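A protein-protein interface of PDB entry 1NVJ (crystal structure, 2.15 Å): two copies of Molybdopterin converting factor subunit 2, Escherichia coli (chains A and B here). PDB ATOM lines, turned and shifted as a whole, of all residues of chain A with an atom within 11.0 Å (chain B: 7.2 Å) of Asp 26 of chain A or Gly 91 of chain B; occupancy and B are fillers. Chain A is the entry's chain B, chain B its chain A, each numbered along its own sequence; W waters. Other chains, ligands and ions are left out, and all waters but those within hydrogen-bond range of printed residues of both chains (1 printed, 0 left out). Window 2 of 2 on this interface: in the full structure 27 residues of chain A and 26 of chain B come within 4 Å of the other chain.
No position is printed for both chains.
The backbone carbonyl oxygen of Ala 102 of chain A sits at hydrogen-bond distance from the guanidinium group of Arg 39 of chain B. NZ of Lys 37 of chain B sits at hydrogen-bond distance from O of Ala 23 of chain A (2.9 Å). The backbone NH of Lys 37 of chain B sits at hydrogen-bond distance from the backbone carbonyl oxygen of Gly 29 of chain A (2.8 Å). The side-chain hydroxyl (OH) of Tyr 19 of chain A sits at hydrogen-bond distance from the side-chain carboxylate (OE2) of Glu 93 of chain B, 2.8 Å away. The side-chain amino group of Lys 37 of chain B sits at hydrogen-bond distance from the backbone carbonyl oxygen of Asp 28 of chain A, at 2.7 Å. The side-chain amino group of Lys 37 of chain B is in hydrogen-bond range of the backbone carbonyl oxygen of Arg 25 of chain A. The guanidinium group (NH1) of Arg 39 of chain B sits at hydrogen-bond distance from the backbone carbonyl oxygen (O) of Gly 29 of chain A (3.2 Å).
OE2 of Glu 93 of chain B touches CB of Ala 23 of chain A, at 3.6 Å. Gly 91 of chain B touches Asp 26 of chain A. Gly 29 of chain A touches Gly 36 of chain B (O to CA, 3.6 Å). Ala 30 of chain A touches Arg 39 of chain B (CB to NH2, 3.9 Å).
Hydrophobic or aromatic side chains of chain A within 4 Å of the printed part of chain B: Tyr 19, Ala 23 and Ala 30. Printed residues of chain B that touch a printed residue of chain A: Gly 36, Lys 37, Arg 39, Gly 91 and Glu 93. Among the printed residues, 11 pairs touch across the chains.
The side-chain hydroxyl of Thr 100 of chain A lies within hydrogen-bond range of the side-chain carboxylate of Asp 28 of chain A, at 3.0 Å. O of Ser 101 of chain A sits at hydrogen-bond distance from N of Ala 30 of chain A. The side-chain carboxylate (OD2) of Asp 28 of chain A is in salt-bridge range of the guanidinium group (NE) of Arg 25 of chain A, at 2.9 Å. The backbone carbonyl oxygen of Ser 101 of chain A sits at hydrogen-bond distance from the backbone NH of Gly 29 of chain A (3.1 Å). O of Gly 36 of chain B sits at hydrogen-bond distance from N of Ile 94 of chain B, 2.9 Å away. The side-chain carboxylate (OE2) of Glu 27 of chain A is in salt-bridge range of the guanidinium group (NH1) of Arg 25 of chain A, at 3.8 Å.
Asp 26 of chain A touches one residue of chain B. Gly 91 of chain B touches just one residue of chain A: Asp 26. Of the printed residues of chain A, Lys 37 of chain B touches Ala 23 (2.9 Å), Arg 25 (2.8 Å), Asp 28 (2.7 Å) and Gly 29 (2.8 Å). No residue of chain A comes within 4 Å of Val 38 of chain B. No residue of chain A comes within 4 Å of Pro 90 of chain B. No residue of chain A comes within 4 Å of Asp 92 of chain B. Of the printed residues of chain B, Ala 30 of chain A touches Arg 39 (3.9 Å). Of the printed residues of chain B, Ala 102 of chain A touches Arg 39. Of the printed residues of chain B, Ala 23 of chain A touches Lys 37 (2.9 Å) and Glu 93 (3.6 Å). Printed residues of chain A within 4 Å of Gly 36 of chain B: Gly 29. Of the printed residues of chain B, Gly 29 of chain A touches Gly 36, Lys 37 and Arg 39. The nearest residue of chain A that does not touch Gly 91 of chain B is Ala 23 of chain A (5.9 Å). The nearest printed residue of chain B that does not touch Arg 25 of chain A is Gly 91 of chain B (6.2 Å).
Water W1 lies within hydrogen-bond range of OE2 of Glu 93 of chain B (2.6 Å) and O of Ala 23 of chain A (2.9 Å).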
ATOM      1  N   GLU A   3     -26.310  20.605  14.520  1.00  0.00           N
ATOM      2  CA  GLU A   3     -26.413  21.758  15.377  1.00  0.00           C
ATOM      3  C   GLU A   3     -25.771  22.998  14.719  1.00  0.00           C
ATOM      4  O   GLU A   3     -24.879  22.868  13.875  1.00  0.00           O
ATOM      5  CB  GLU A   3     -25.772  21.413  16.728  1.00  0.00           C
ATOM      6  CG  GLU A   3     -26.488  20.280  17.470  1.00  0.00           C
ATOM      7  CD  GLU A   3     -25.854  18.892  17.281  1.00  0.00           C
ATOM      8  OE1 GLU A   3     -25.318  18.558  16.197  1.00  0.00           O
ATOM      9  OE2 GLU A   3     -25.897  18.101  18.242  1.00  0.00           O
ATOM     10  N   TYR A  19     -13.026  24.618  17.776  1.00  0.00           N
ATOM     11  CA  TYR A  19     -12.835  23.604  16.747  1.00  0.00           C
ATOM     12  C   TYR A  19     -13.285  22.206  17.197  1.00  0.00           C
ATOM     13  O   TYR A  19     -13.939  21.517  16.415  1.00  0.00           O
ATOM     14  CB  TYR A  19     -11.388  23.602  16.200  1.00  0.00           C
ATOM     15  CG  TYR A  19     -11.139  22.495  15.217  1.00  0.00           C
ATOM     16  CD1 TYR A  19     -11.271  22.702  13.847  1.00  0.00           C
ATOM     17  CD2 TYR A  19     -10.803  21.216  15.664  1.00  0.00           C
ATOM     18  CE1 TYR A  19     -11.068  21.648  12.940  1.00  0.00           C
ATOM     19  CE2 TYR A  19     -10.605  20.176  14.786  1.00  0.00           C
ATOM     20  CZ  TYR A  19     -10.742  20.387  13.426  1.00  0.00           C
ATOM     21  OH  TYR A  19     -10.514  19.328  12.564  1.00  0.00           O
ATOM     22  N   PRO A  20     -12.952  21.769  18.411  1.00  0.00           N
ATOM     23  CA  PRO A  20     -13.339  20.429  18.876  1.00  0.00           C
ATOM     24  C   PRO A  20     -14.850  20.137  18.842  1.00  0.00           C
ATOM     25  O   PRO A  20     -15.229  19.046  18.421  1.00  0.00           O
ATOM     26  CB  PRO A  20     -12.786  20.393  20.300  1.00  0.00           C
ATOM     27  CG  PRO A  20     -11.636  21.301  20.246  1.00  0.00           C
ATOM     28  CD  PRO A  20     -12.133  22.450  19.426  1.00  0.00           C
ATOM     29  N   TRP A  21     -15.696  21.086  19.231  1.00  0.00           N
ATOM     30  CA  TRP A  21     -17.124  20.884  19.093  1.00  0.00           C
ATOM     31  C   TRP A  21     -17.476  20.791  17.605  1.00  0.00           C
ATOM     32  O   TRP A  21     -18.299  19.968  17.195  1.00  0.00           O
ATOM     33  CB  TRP A  21     -17.925  22.011  19.764  1.00  0.00           C
ATOM     34  CG  TRP A  21     -19.412  21.841  19.689  1.00  0.00           C
ATOM     35  CD1 TRP A  21     -20.207  21.132  20.559  1.00  0.00           C
ATOM     36  CD2 TRP A  21     -20.310  22.406  18.713  1.00  0.00           C
ATOM     37  NE1 TRP A  21     -21.526  21.216  20.177  1.00  0.00           N
ATOM     38  CE2 TRP A  21     -21.619  22.000  19.056  1.00  0.00           C
ATOM     39  CE3 TRP A  21     -20.144  23.226  17.600  1.00  0.00           C
ATOM     40  CZ2 TRP A  21     -22.739  22.364  18.309  1.00  0.00           C
ATOM     41  CZ3 TRP A  21     -21.251  23.585  16.853  1.00  0.00           C
ATOM     42  CH2 TRP A  21     -22.541  23.152  17.208  1.00  0.00           C
ATOM     43  N   LEU A  22     -16.852  21.627  16.795  1.00  0.00           N
ATOM     44  CA  LEU A  22     -17.244  21.730  15.397  1.00  0.00           C
ATOM     45  C   LEU A  22     -16.971  20.415  14.696  1.00  0.00           C
ATOM     46  O   LEU A  22     -17.763  19.973  13.860  1.00  0.00           O
ATOM     47  CB  LEU A  22     -16.536  22.912  14.714  1.00  0.00           C
ATOM     48  CG  LEU A  22     -16.771  23.104  13.225  1.00  0.00           C
ATOM     49  CD1 LEU A  22     -18.200  23.538  12.948  1.00  0.00           C
ATOM     50  CD2 LEU A  22     -15.765  24.097  12.665  1.00  0.00           C
ATOM     51  N   ALA A  23     -15.878  19.763  15.077  1.00  0.00           N
ATOM     52  CA  ALA A  23     -15.381  18.602  14.362  1.00  0.00           C
ATOM     53  C   ALA A  23     -15.696  17.295  15.078  1.00  0.00           C
ATOM     54  O   ALA A  23     -15.159  16.250  14.720  1.00  0.00           O
ATOM     55  CB  ALA A  23     -13.875  18.738  14.144  1.00  0.00           C
ATOM     56  N   GLU A  24     -16.591  17.347  16.064  1.00  0.00           N
ATOM     57  CA  GLU A  24     -16.805  16.199  16.928  1.00  0.00           C
ATOM     58  C   GLU A  24     -17.423  14.996  16.234  1.00  0.00           C
ATOM     59  O   GLU A  24     -17.032  13.888  16.521  1.00  0.00           O
ATOM     60  CB  GLU A  24     -17.672  16.584  18.135  1.00  0.00           C
ATOM     61  CG  GLU A  24     -18.034  15.411  19.044  1.00  0.00           C
ATOM     62  CD  GLU A  24     -18.658  15.852  20.356  1.00  0.00           C
ATOM     63  OE1 GLU A  24     -19.062  17.039  20.468  1.00  0.00           O
ATOM     64  OE2 GLU A  24     -18.734  15.003  21.282  1.00  0.00           O
ATOM     65  N   ARG A  25     -18.408  15.208  15.368  1.00  0.00           N
ATOM     66  CA  ARG A  25     -19.226  14.104  14.849  1.00  0.00           C
ATOM     67  C   ARG A  25     -18.494  13.319  13.774  1.00  0.00           C
ATOM     68  O   ARG A  25     -17.925  13.923  12.854  1.00  0.00           O
ATOM     69  CB  ARG A  25     -20.513  14.657  14.241  1.00  0.00           C
ATOM     70  CG  ARG A  25     -21.336  15.541  15.184  1.00  0.00           C
ATOM     71  CD  ARG A  25     -22.787  15.786  14.743  1.00  0.00           C
ATOM     72  NE  ARG A  25     -22.928  16.050  13.301  1.00  0.00           N
ATOM     73  CZ  ARG A  25     -24.094  16.058  12.645  1.00  0.00           C
ATOM     74  NH1 ARG A  25     -25.240  15.825  13.285  1.00  0.00           N
ATOM     75  NH2 ARG A  25     -24.120  16.268  11.334  1.00  0.00           N
ATOM     76  N   ASP A  26     -18.520  11.986  13.859  1.00  0.00           N
ATOM     77  CA  ASP A  26     -17.876  11.138  12.842  1.00  0.00           C
ATOM     78  C   ASP A  26     -18.463  11.340  11.426  1.00  0.00           C
ATOM     79  O   ASP A  26     -17.713  11.391  10.444  1.00  0.00           O
ATOM     80  CB  ASP A  26     -17.910   9.650  13.242  1.00  0.00           C
ATOM     81  CG  ASP A  26     -17.058   9.344  14.486  1.00  0.00           C
ATOM     82  OD1 ASP A  26     -16.295  10.222  14.957  1.00  0.00           O
ATOM     83  OD2 ASP A  26     -17.098   8.249  15.070  1.00  0.00           O
ATOM     84  N   GLU A  27     -19.780  11.493  11.315  1.00  0.00           N
ATOM     85  CA  GLU A  27     -20.424  11.756  10.020  1.00  0.00           C
ATOM     86  C   GLU A  27     -20.022  13.095   9.377  1.00  0.00           C
ATOM     87  O   GLU A  27     -20.263  13.324   8.176  1.00  0.00           O
ATOM     88  CB  GLU A  27     -21.952  11.706  10.164  1.00  0.00           C
ATOM     89  CG  GLU A  27     -22.539  12.749  11.113  1.00  0.00           C
ATOM     90  CD  GLU A  27     -23.074  12.144  12.410  1.00  0.00           C
ATOM     91  OE1 GLU A  27     -22.256  11.639  13.216  1.00  0.00           O
ATOM     92  OE2 GLU A  27     -24.317  12.177  12.619  1.00  0.00           O
ATOM     93  N   ASP A  28     -19.455  14.000  10.167  1.00  0.00           N
ATOM     94  CA  ASP A  28     -18.902  15.234   9.633  1.00  0.00           C
ATOM     95  C   ASP A  28     -17.436  15.004   9.218  1.00  0.00           C
ATOM     96  O   ASP A  28     -16.510  15.357   9.946  1.00  0.00           O
ATOM     97  CB  ASP A  28     -19.009  16.348  10.673  1.00  0.00           C
ATOM     98  CG  ASP A  28     -20.450  16.763  10.954  1.00  0.00           C
ATOM     99  OD1 ASP A  28     -21.367  16.350  10.204  1.00  0.00           O
ATOM    100  OD2 ASP A  28     -20.757  17.487  11.940  1.00  0.00           O
ATOM    101  N   GLY A  29     -17.246  14.428   8.032  1.00  0.00           N
ATOM    102  CA  GLY A  29     -15.930  14.018   7.558  1.00  0.00           C
ATOM    103  C   GLY A  29     -15.019  15.119   7.010  1.00  0.00           C
ATOM    104  O   GLY A  29     -13.802  14.939   6.928  1.00  0.00           O
ATOM    105  N   ALA A  30     -15.624  16.245   6.633  1.00  0.00           N
ATOM    106  CA  ALA A  30     -14.928  17.376   6.063  1.00  0.00           C
ATOM    107  C   ALA A  30     -15.233  18.593   6.915  1.00  0.00           C
ATOM    108  O   ALA A  30     -16.401  18.896   7.172  1.00  0.00           O
ATOM    109  CB  ALA A  30     -15.379  17.591   4.630  1.00  0.00           C
ATOM    110  N   VAL A  31     -14.178  19.265   7.381  1.00  0.00           N
ATOM    111  CA  VAL A  31     -14.304  20.429   8.274  1.00  0.00           C
ATOM    112  C   VAL A  31     -13.556  21.611   7.693  1.00  0.00           C
ATOM    113  O   VAL A  31     -12.344  21.541   7.493  1.00  0.00           O
ATOM    114  CB  VAL A  31     -13.704  20.151   9.646  1.00  0.00           C
ATOM    115  CG1 VAL A  31     -13.976  21.353  10.610  1.00  0.00           C
ATOM    116  CG2 VAL A  31     -14.264  18.861  10.216  1.00  0.00           C
ATOM    117  N   GLY A  77     -23.386  19.568   8.224  1.00  0.00           N
ATOM    118  CA  GLY A  77     -23.525  19.079   9.582  1.00  0.00           C
ATOM    119  C   GLY A  77     -23.462  20.246  10.564  1.00  0.00           C
ATOM    120  O   GLY A  77     -24.255  21.188  10.479  1.00  0.00           O
ATOM    121  N   ARG A  78     -22.537  20.180  11.513  1.00  0.00           N
ATOM    122  CA  ARG A  78     -22.381  21.258  12.479  1.00  0.00           C
ATOM    123  C   ARG A  78     -21.819  22.503  11.792  1.00  0.00           C
ATOM    124  O   ARG A  78     -20.949  22.419  10.897  1.00  0.00           O
ATOM    125  CB  ARG A  78     -21.504  20.831  13.638  1.00  0.00           C
ATOM    126  CG  ARG A  78     -22.244  19.962  14.629  1.00  0.00           C
ATOM    127  CD  ARG A  78     -21.491  19.737  15.939  1.00  0.00           C
ATOM    128  NE  ARG A  78     -22.302  18.972  16.868  1.00  0.00           N
ATOM    129  CZ  ARG A  78     -21.855  18.398  17.972  1.00  0.00           C
ATOM    130  NH1 ARG A  78     -20.592  18.508  18.331  1.00  0.00           N
ATOM    131  NH2 ARG A  78     -22.690  17.702  18.725  1.00  0.00           N
ATOM    132  N   THR A 100     -19.180  21.928   8.485  1.00  0.00           N
ATOM    133  CA  THR A 100     -18.836  20.565   8.193  1.00  0.00           C
ATOM    134  C   THR A 100     -19.784  19.975   7.164  1.00  0.00           C
ATOM    135  O   THR A 100     -20.889  20.485   6.928  1.00  0.00           O
ATOM    136  CB  THR A 100     -18.888  19.681   9.434  1.00  0.00           C
ATOM    137  OG1 THR A 100     -20.231  19.628   9.940  1.00  0.00           O
ATOM    138  CG2 THR A 100     -18.041  20.229  10.534  1.00  0.00           C
ATOM    139  N   SER A 101     -19.335  18.863   6.606  1.00  0.00           N
ATOM    140  CA  SER A 101     -20.042  18.164   5.550  1.00  0.00           C
ATOM    141  C   SER A 101     -19.424  16.772   5.357  1.00  0.00           C
ATOM    142  O   SER A 101     -18.411  16.444   5.944  1.00  0.00           O
ATOM    143  CB  SER A 101     -19.982  18.984   4.260  1.00  0.00           C
ATOM    144  OG  SER A 101     -20.758  18.395   3.245  1.00  0.00           O
ATOM    145  N   ALA A 102     -20.070  15.947   4.551  1.00  0.00           N
ATOM    146  CA  ALA A 102     -19.509  14.668   4.160  1.00  0.00           C
ATOM    147  C   ALA A 102     -18.515  14.901   3.026  1.00  0.00           C
ATOM    148  O   ALA A 102     -17.540  14.184   2.903  1.00  0.00           O
ATOM    149  CB  ALA A 102     -20.636  13.701   3.719  1.00  0.00           C
ATOM    150  N   HIS A 103     -18.775  15.915   2.206  1.00  0.00           N
ATOM    151  CA  HIS A 103     -17.922  16.237   1.056  1.00  0.00           C
ATOM    152  C   HIS A 103     -17.191  17.573   1.250  1.00  0.00           C
ATOM    153  O   HIS A 103     -17.787  18.536   1.701  1.00  0.00           O
ATOM    154  CB  HIS A 103     -18.776  16.272  -0.232  1.00  0.00           C
ATOM    155  CG  HIS A 103     -19.832  15.213  -0.273  1.00  0.00           C
ATOM    156  ND1 HIS A 103     -19.541  13.884  -0.503  1.00  0.00           N
ATOM    157  CD2 HIS A 103     -21.173  15.283  -0.085  1.00  0.00           C
ATOM    158  CE1 HIS A 103     -20.659  13.179  -0.448  1.00  0.00           C
ATOM    159  NE2 HIS A 103     -21.663  14.004  -0.198  1.00  0.00           N
ATOM    160  N   GLY B  36      -9.631  16.742   6.872  1.00  0.00           N
ATOM    161  CA  GLY B  36     -10.275  15.553   6.346  1.00  0.00           C
ATOM    162  C   GLY B  36     -10.204  14.414   7.341  1.00  0.00           C
ATOM    163  O   GLY B  36      -9.175  14.192   7.957  1.00  0.00           O
ATOM    164  N   LYS B  37     -11.319  13.707   7.514  1.00  0.00           N
ATOM    165  CA  LYS B  37     -11.391  12.575   8.425  1.00  0.00           C
ATOM    166  C   LYS B  37     -11.613  11.302   7.649  1.00  0.00           C
ATOM    167  O   LYS B  37     -12.002  11.341   6.490  1.00  0.00           O
ATOM    168  CB  LYS B  37     -12.517  12.774   9.433  1.00  0.00           C
ATOM    169  CG  LYS B  37     -12.137  13.736  10.522  1.00  0.00           C
ATOM    170  CD  LYS B  37     -13.307  14.626  10.955  1.00  0.00           C
ATOM    171  CE  LYS B  37     -14.300  13.865  11.757  1.00  0.00           C
ATOM    172  NZ  LYS B  37     -15.310  14.797  12.251  1.00  0.00           N
ATOM    173  N   VAL B  38     -11.325  10.183   8.299  1.00  0.00           N
ATOM    174  CA  VAL B  38     -11.615   8.868   7.755  1.00  0.00           C
ATOM    175  C   VAL B  38     -13.133   8.730   7.735  1.00  0.00           C
ATOM    176  O   VAL B  38     -13.786   8.878   8.776  1.00  0.00           O
ATOM    177  CB  VAL B  38     -10.996   7.731   8.623  1.00  0.00           C
ATOM    178  CG1 VAL B  38     -11.416   6.354   8.088  1.00  0.00           C
ATOM    179  CG2 VAL B  38      -9.463   7.858   8.704  1.00  0.00           C
ATOM    180  N   ARG B  39     -13.682   8.444   6.550  1.00  0.00           N
ATOM    181  CA  ARG B  39     -15.136   8.517   6.312  1.00  0.00           C
ATOM    182  C   ARG B  39     -15.826   7.187   6.613  1.00  0.00           C
ATOM    183  O   ARG B  39     -15.347   6.410   7.446  1.00  0.00           O
ATOM    184  CB  ARG B  39     -15.422   8.923   4.860  1.00  0.00           C
ATOM    185  CG  ARG B  39     -14.697  10.172   4.403  1.00  0.00           C
ATOM    186  CD  ARG B  39     -15.259  11.460   4.979  1.00  0.00           C
ATOM    187  NE  ARG B  39     -15.300  12.522   3.975  1.00  0.00           N
ATOM    188  CZ  ARG B  39     -14.278  13.327   3.667  1.00  0.00           C
ATOM    189  NH1 ARG B  39     -13.091  13.217   4.270  1.00  0.00           N
ATOM    190  NH2 ARG B  39     -14.448  14.257   2.729  1.00  0.00           N
ATOM    191  N   LEU B  88      -5.333   3.809  11.067  1.00  0.00           N
ATOM    192  CA  LEU B  88      -6.337   4.855  11.225  1.00  0.00           C
ATOM    193  C   LEU B  88      -7.776   4.331  11.230  1.00  0.00           C
ATOM    194  O   LEU B  88      -8.135   3.431  10.462  1.00  0.00           O
ATOM    195  CB  LEU B  88      -6.186   5.899  10.126  1.00  0.00           C
ATOM    196  CG  LEU B  88      -4.832   6.588  10.050  1.00  0.00           C
ATOM    197  CD1 LEU B  88      -4.683   7.211   8.676  1.00  0.00           C
ATOM    198  CD2 LEU B  88      -4.697   7.599  11.173  1.00  0.00           C
ATOM    199  N   TRP B  89      -8.592   4.939  12.089  1.00  0.00           N
ATOM    200  CA  TRP B  89      -9.928   4.456  12.397  1.00  0.00           C
ATOM    201  C   TRP B  89     -10.955   5.515  12.105  1.00  0.00           C
ATOM    202  O   TRP B  89     -10.637   6.695  12.117  1.00  0.00           O
ATOM    203  CB  TRP B  89     -10.000   4.120  13.882  1.00  0.00           C
ATOM    204  CG  TRP B  89      -9.076   3.034  14.246  1.00  0.00           C
ATOM    205  CD1 TRP B  89      -7.761   3.153  14.576  1.00  0.00           C
ATOM    206  CD2 TRP B  89      -9.386   1.646  14.296  1.00  0.00           C
ATOM    207  NE1 TRP B  89      -7.225   1.915  14.828  1.00  0.00           N
ATOM    208  CE2 TRP B  89      -8.203   0.969  14.664  1.00  0.00           C
ATOM    209  CE3 TRP B  89     -10.549   0.897  14.068  1.00  0.00           C
ATOM    210  CZ2 TRP B  89      -8.151  -0.415  14.813  1.00  0.00           C
ATOM    211  CZ3 TRP B  89     -10.500  -0.475  14.214  1.00  0.00           C
ATOM    212  CH2 TRP B  89      -9.308  -1.119  14.586  1.00  0.00           C
ATOM    213  N   PRO B  90     -12.202   5.107  11.880  1.00  0.00           N
ATOM    214  CA  PRO B  90     -13.278   6.071  11.654  1.00  0.00           C
ATOM    215  C   PRO B  90     -13.217   7.261  12.625  1.00  0.00           C
ATOM    216  O   PRO B  90     -13.013   7.080  13.831  1.00  0.00           O
ATOM    217  CB  PRO B  90     -14.554   5.248  11.882  1.00  0.00           C
ATOM    218  CG  PRO B  90     -14.094   3.858  12.308  1.00  0.00           C
ATOM    219  CD  PRO B  90     -12.695   3.718  11.816  1.00  0.00           C
ATOM    220  N   GLY B  91     -13.363   8.464  12.072  1.00  0.00           N
ATOM    221  CA  GLY B  91     -13.417   9.684  12.852  1.00  0.00           C
ATOM    222  C   GLY B  91     -12.063  10.277  13.183  1.00  0.00           C
ATOM    223  O   GLY B  91     -12.012  11.350  13.777  1.00  0.00           O
ATOM    224  N   ASP B  92     -10.986   9.578  12.828  1.00  0.00           N
ATOM    225  CA  ASP B  92      -9.629  10.093  12.962  1.00  0.00           C
ATOM    226  C   ASP B  92      -9.429  11.175  11.917  1.00  0.00           C
ATOM    227  O   ASP B  92      -9.786  11.008  10.742  1.00  0.00           O
ATOM    228  CB  ASP B  92      -8.574   8.998  12.722  1.00  0.00           C
ATOM    229  CG  ASP B  92      -8.318   8.132  13.944  1.00  0.00           C
ATOM    230  OD1 ASP B  92      -8.793   8.497  15.029  1.00  0.00           O
ATOM    231  OD2 ASP B  92      -7.634   7.076  13.916  1.00  0.00           O
ATOM    232  N   GLU B  93      -8.847  12.278  12.359  1.00  0.00           N
ATOM    233  CA  GLU B  93      -8.502  13.393  11.500  1.00  0.00           C
ATOM    234  C   GLU B  93      -7.164  13.059  10.855  1.00  0.00           C
ATOM    235  O   GLU B  93      -6.175  12.892  11.561  1.00  0.00           O
ATOM    236  CB  GLU B  93      -8.417  14.660  12.328  1.00  0.00           C
ATOM    237  CG  GLU B  93      -9.748  15.036  12.952  1.00  0.00           C
ATOM    238  CD  GLU B  93      -9.674  16.272  13.826  1.00  0.00           C
ATOM    239  OE1 GLU B  93      -8.568  16.585  14.320  1.00  0.00           O
ATOM    240  OE2 GLU B  93     -10.717  16.931  14.024  1.00  0.00           O
ATOM    241  N   ILE B  94      -7.140  12.943   9.524  1.00  0.00           N
ATOM    242  CA  ILE B  94      -5.962  12.428   8.829  1.00  0.00           C
ATOM    243  C   ILE B  94      -5.198  13.472   8.015  1.00  0.00           C
ATOM    244  O   ILE B  94      -3.976  13.326   7.793  1.00  0.00           O
ATOM    245  CB  ILE B  94      -6.323  11.161   7.989  1.00  0.00           C
ATOM    246  CG1 ILE B  94      -7.518  11.379   7.062  1.00  0.00           C
ATOM    247  CG2 ILE B  94      -6.686  10.038   8.924  1.00  0.00           C
ATOM    248  CD1 ILE B  94      -7.544  10.429   5.872  1.00  0.00           C
HETATM  249  O   HOH W   1     -12.450  15.236  14.875  1.00  0.00           O
